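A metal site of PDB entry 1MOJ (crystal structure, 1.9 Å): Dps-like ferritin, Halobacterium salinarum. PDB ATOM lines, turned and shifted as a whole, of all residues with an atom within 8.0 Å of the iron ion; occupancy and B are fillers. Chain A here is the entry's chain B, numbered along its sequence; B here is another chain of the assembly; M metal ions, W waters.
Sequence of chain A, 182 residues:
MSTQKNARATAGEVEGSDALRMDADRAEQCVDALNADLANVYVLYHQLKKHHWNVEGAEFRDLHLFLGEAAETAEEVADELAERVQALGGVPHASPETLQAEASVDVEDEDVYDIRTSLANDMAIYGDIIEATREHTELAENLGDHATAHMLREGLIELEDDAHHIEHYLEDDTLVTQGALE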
ATOM      1  N   GLU A  75      11.685  19.640  35.812  1.00  0.00           N
ATOM      2  CA  GLU A  75      12.811  19.660  34.887  1.00  0.00           C
ATOM      3  C   GLU A  75      12.601  18.714  33.703  1.00  0.00           C
ATOM      4  O   GLU A  75      13.011  19.020  32.580  1.00  0.00           O
ATOM      5  CB  GLU A  75      14.099  19.289  35.617  1.00  0.00           C
ATOM      6  CG  GLU A  75      15.336  19.874  34.977  1.00  0.00           C
ATOM      7  CD  GLU A  75      16.281  18.811  34.471  1.00  0.00           C
ATOM      8  OE1 GLU A  75      15.848  17.992  33.640  1.00  0.00           O
ATOM      9  OE2 GLU A  75      17.457  18.808  34.911  1.00  0.00           O
ATOM     10  N   GLU A  76      11.954  17.581  33.954  1.00  0.00           N
ATOM     11  CA  GLU A  76      11.674  16.626  32.896  1.00  0.00           C
ATOM     12  C   GLU A  76      10.588  17.167  31.965  1.00  0.00           C
ATOM     13  O   GLU A  76      10.655  16.981  30.751  1.00  0.00           O
ATOM     14  CB  GLU A  76      11.232  15.299  33.507  1.00  0.00           C
ATOM     15  CG  GLU A  76      12.363  14.568  34.214  1.00  0.00           C
ATOM     16  CD  GLU A  76      11.964  13.179  34.707  1.00  0.00           C
ATOM     17  OE1 GLU A  76      11.161  12.511  34.006  1.00  0.00           O
ATOM     18  OE2 GLU A  76      12.474  12.752  35.772  1.00  0.00           O
ATOM     19  N   ALA A  78      10.014  20.324  31.382  1.00  0.00           N
ATOM     20  CA  ALA A  78      10.672  21.378  30.597  1.00  0.00           C
ATOM     21  C   ALA A  78      11.463  20.763  29.449  1.00  0.00           C
ATOM     22  O   ALA A  78      11.444  21.258  28.329  1.00  0.00           O
ATOM     23  CB  ALA A  78      11.603  22.208  31.475  1.00  0.00           C
ATOM     24  N   ASP A  79      12.161  19.667  29.733  1.00  0.00           N
ATOM     25  CA  ASP A  79      12.949  18.971  28.719  1.00  0.00           C
ATOM     26  C   ASP A  79      12.027  18.484  27.594  1.00  0.00           C
ATOM     27  O   ASP A  79      12.333  18.630  26.413  1.00  0.00           O
ATOM     28  CB  ASP A  79      13.694  17.787  29.338  1.00  0.00           C
ATOM     29  CG  ASP A  79      14.716  17.194  28.397  1.00  0.00           C
ATOM     30  OD1 ASP A  79      15.709  17.888  28.079  1.00  0.00           O
ATOM     31  OD2 ASP A  79      14.530  16.036  27.977  1.00  0.00           O
ATOM     32  N   GLU A  80      10.902  17.912  27.977  1.00  0.00           N
ATOM     33  CA  GLU A  80       9.923  17.439  27.003  1.00  0.00           C
ATOM     34  C   GLU A  80       9.449  18.594  26.131  1.00  0.00           C
ATOM     35  O   GLU A  80       9.438  18.501  24.906  1.00  0.00           O
ATOM     36  CB  GLU A  80       8.727  16.841  27.718  1.00  0.00           C
ATOM     37  CG  GLU A  80       8.985  15.505  28.401  1.00  0.00           C
ATOM     38  CD  GLU A  80       9.157  14.374  27.407  1.00  0.00           C
ATOM     39  OE1 GLU A  80       8.915  13.209  27.786  1.00  0.00           O
ATOM     40  OE2 GLU A  80       9.544  14.634  26.245  1.00  0.00           O
ATOM     41  N   ALA A  82      10.798  21.668  25.657  1.00  0.00           N
ATOM     42  CA  ALA A  82      11.884  22.219  24.871  1.00  0.00           C
ATOM     43  C   ALA A  82      12.187  21.368  23.647  1.00  0.00           C
ATOM     44  O   ALA A  82      12.388  21.877  22.539  1.00  0.00           O
ATOM     45  CB  ALA A  82      13.110  22.362  25.708  1.00  0.00           C
ATOM     46  N   GLU A  83      12.238  20.051  23.842  1.00  0.00           N
ATOM     47  CA  GLU A  83      12.529  19.154  22.743  1.00  0.00           C
ATOM     48  C   GLU A  83      11.396  19.106  21.728  1.00  0.00           C
ATOM     49  O   GLU A  83      11.644  18.944  20.534  1.00  0.00           O
ATOM     50  CB  GLU A  83      12.851  17.752  23.268  1.00  0.00           C
ATOM     51  CG  GLU A  83      14.202  17.724  23.995  1.00  0.00           C
ATOM     52  CD  GLU A  83      14.622  16.336  24.445  1.00  0.00           C
ATOM     53  OE1 GLU A  83      15.728  16.229  25.014  1.00  0.00           O
ATOM     54  OE2 GLU A  83      13.865  15.366  24.237  1.00  0.00           O
ATOM     55  N   LYS B  49      21.943  22.245  28.208  1.00  0.00           N
ATOM     56  CA  LYS B  49      20.605  21.790  27.865  1.00  0.00           C
ATOM     57  C   LYS B  49      20.254  22.310  26.490  1.00  0.00           C
ATOM     58  O   LYS B  49      19.739  21.574  25.641  1.00  0.00           O
ATOM     59  CB  LYS B  49      19.583  22.322  28.873  1.00  0.00           C
ATOM     60  CG  LYS B  49      19.757  21.758  30.263  1.00  0.00           C
ATOM     61  CD  LYS B  49      18.599  20.866  30.667  1.00  0.00           C
ATOM     62  CE  LYS B  49      18.425  19.683  29.755  1.00  0.00           C
ATOM     63  NZ  LYS B  49      17.486  18.692  30.380  1.00  0.00           N
ATOM     64  N   HIS B  52      22.039  20.399  23.908  1.00  0.00           N
ATOM     65  CA  HIS B  52      21.495  19.047  23.965  1.00  0.00           C
ATOM     66  C   HIS B  52      20.218  19.034  23.092  1.00  0.00           C
ATOM     67  O   HIS B  52      20.043  18.182  22.226  1.00  0.00           O
ATOM     68  CB  HIS B  52      21.165  18.750  25.438  1.00  0.00           C
ATOM     69  CG  HIS B  52      20.230  17.601  25.650  1.00  0.00           C
ATOM     70  ND1 HIS B  52      20.601  16.287  25.483  1.00  0.00           N
ATOM     71  CD2 HIS B  52      18.956  17.572  26.116  1.00  0.00           C
ATOM     72  CE1 HIS B  52      19.609  15.494  25.841  1.00  0.00           C
ATOM     73  NE2 HIS B  52      18.594  16.252  26.224  1.00  0.00           N
ATOM     74  N   TRP B  53      19.332  20.002  23.327  1.00  0.00           N
ATOM     75  CA  TRP B  53      18.083  20.099  22.578  1.00  0.00           C
ATOM     76  C   TRP B  53      18.284  20.356  21.094  1.00  0.00           C
ATOM     77  O   TRP B  53      17.671  19.712  20.265  1.00  0.00           O
ATOM     78  CB  TRP B  53      17.187  21.237  23.113  1.00  0.00           C
ATOM     79  CG  TRP B  53      16.777  21.154  24.558  1.00  0.00           C
ATOM     80  CD1 TRP B  53      16.483  20.018  25.279  1.00  0.00           C
ATOM     81  CD2 TRP B  53      16.581  22.262  25.454  1.00  0.00           C
ATOM     82  NE1 TRP B  53      16.111  20.360  26.569  1.00  0.00           N
ATOM     83  CE2 TRP B  53      16.166  21.723  26.699  1.00  0.00           C
ATOM     84  CE3 TRP B  53      16.718  23.652  25.325  1.00  0.00           C
ATOM     85  CZ2 TRP B  53      15.887  22.533  27.812  1.00  0.00           C
ATOM     86  CZ3 TRP B  53      16.441  24.456  26.430  1.00  0.00           C
ATOM     87  CH2 TRP B  53      16.033  23.892  27.655  1.00  0.00           C
ATOM     88  N   HIS B  64      23.899  14.515  21.569  1.00  0.00           N
ATOM     89  CA  HIS B  64      22.652  14.745  22.287  1.00  0.00           C
ATOM     90  C   HIS B  64      22.742  14.024  23.635  1.00  0.00           C
ATOM     91  O   HIS B  64      22.452  14.603  24.682  1.00  0.00           O
ATOM     92  CB  HIS B  64      21.490  14.168  21.473  1.00  0.00           C
ATOM     93  CG  HIS B  64      20.157  14.307  22.137  1.00  0.00           C
ATOM     94  ND1 HIS B  64      19.543  15.529  22.329  1.00  0.00           N
ATOM     95  CD2 HIS B  64      19.298  13.377  22.612  1.00  0.00           C
ATOM     96  CE1 HIS B  64      18.363  15.339  22.902  1.00  0.00           C
ATOM     97  NE2 HIS B  64      18.188  14.043  23.089  1.00  0.00           N
ATOM     98  N   LEU B  65      23.157  12.763  23.590  1.00  0.00           N
ATOM     99  CA  LEU B  65      23.291  11.946  24.802  1.00  0.00           C
ATOM    100  C   LEU B  65      24.402  12.474  25.710  1.00  0.00           C
ATOM    101  O   LEU B  65      24.250  12.557  26.923  1.00  0.00           O
ATOM    102  CB  LEU B  65      23.556  10.480  24.411  1.00  0.00           C
ATOM    103  CG  LEU B  65      22.427   9.832  23.597  1.00  0.00           C
ATOM    104  CD1 LEU B  65      22.818   8.421  23.173  1.00  0.00           C
ATOM    105  CD2 LEU B  65      21.155   9.787  24.419  1.00  0.00           C
ATOM    106  N   LEU B  67      25.674  15.588  25.854  1.00  0.00           N
ATOM    107  CA  LEU B  67      25.256  16.876  26.382  1.00  0.00           C
ATOM    108  C   LEU B  67      24.189  16.731  27.468  1.00  0.00           C
ATOM    109  O   LEU B  67      24.182  17.486  28.433  1.00  0.00           O
ATOM    110  CB  LEU B  67      24.747  17.756  25.229  1.00  0.00           C
ATOM    111  CG  LEU B  67      25.854  18.228  24.294  1.00  0.00           C
ATOM    112  CD1 LEU B  67      25.270  18.878  23.070  1.00  0.00           C
ATOM    113  CD2 LEU B  67      26.772  19.202  25.024  1.00  0.00           C
ATOM    114  N   GLY B  68      23.289  15.761  27.295  1.00  0.00           N
ATOM    115  CA  GLY B  68      22.266  15.521  28.291  1.00  0.00           C
ATOM    116  C   GLY B  68      22.920  15.080  29.595  1.00  0.00           C
ATOM    117  O   GLY B  68      22.537  15.521  30.680  1.00  0.00           O
HETATM  118 FE    FE M   1      16.434  15.689  26.857  1.00  0.00          FE
HETATM  119  O   HOH W   1      17.190  15.263  29.172  1.00  0.00           O
HETATM  120  O   HOH W   2      16.810  13.738  26.332  1.00  0.00           O
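The side-chain carboxylate (OD1) of Asp 79 is in salt-bridge range of the side-chain amino group (NZ) of Lys 49 of chain B (3.0 Å).
O of His 64 of chain B is in hydrogen-bond range of ND1 of His 52 of chain B (2.6 Å).
The side-chain carboxylate (OD1) of Asp 79 lies within hydrogen-bond range of the indole nitrogen (NE1) of Trp 53 of chain B, 2.9 Å away.
A ring nitrogen (ND1) of His 52 of chain B lies within hydrogen-bond range of the backbone NH (N) of Gly 68 of chain B (3.3 Å).
Of the 14 residues printed, 3 come within 4 Å of the iron ion.
The nearest printed residue that does not touch the iron ion is His 64 of chain B (4.4 Å).
The iron ion is bound by the side-chain carboxylate of Glu 83 (2.0 Å), water W2 (2.1 Å), the side-chain carboxylate of Asp 79 (2.2 Å), a ring nitrogen (NE2) of His 52 of chain B (2.3 Å) and water W1 (2.5 Å).
Slightly farther from the iron ion lies OD1 of Asp 79 (2.6 Å).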
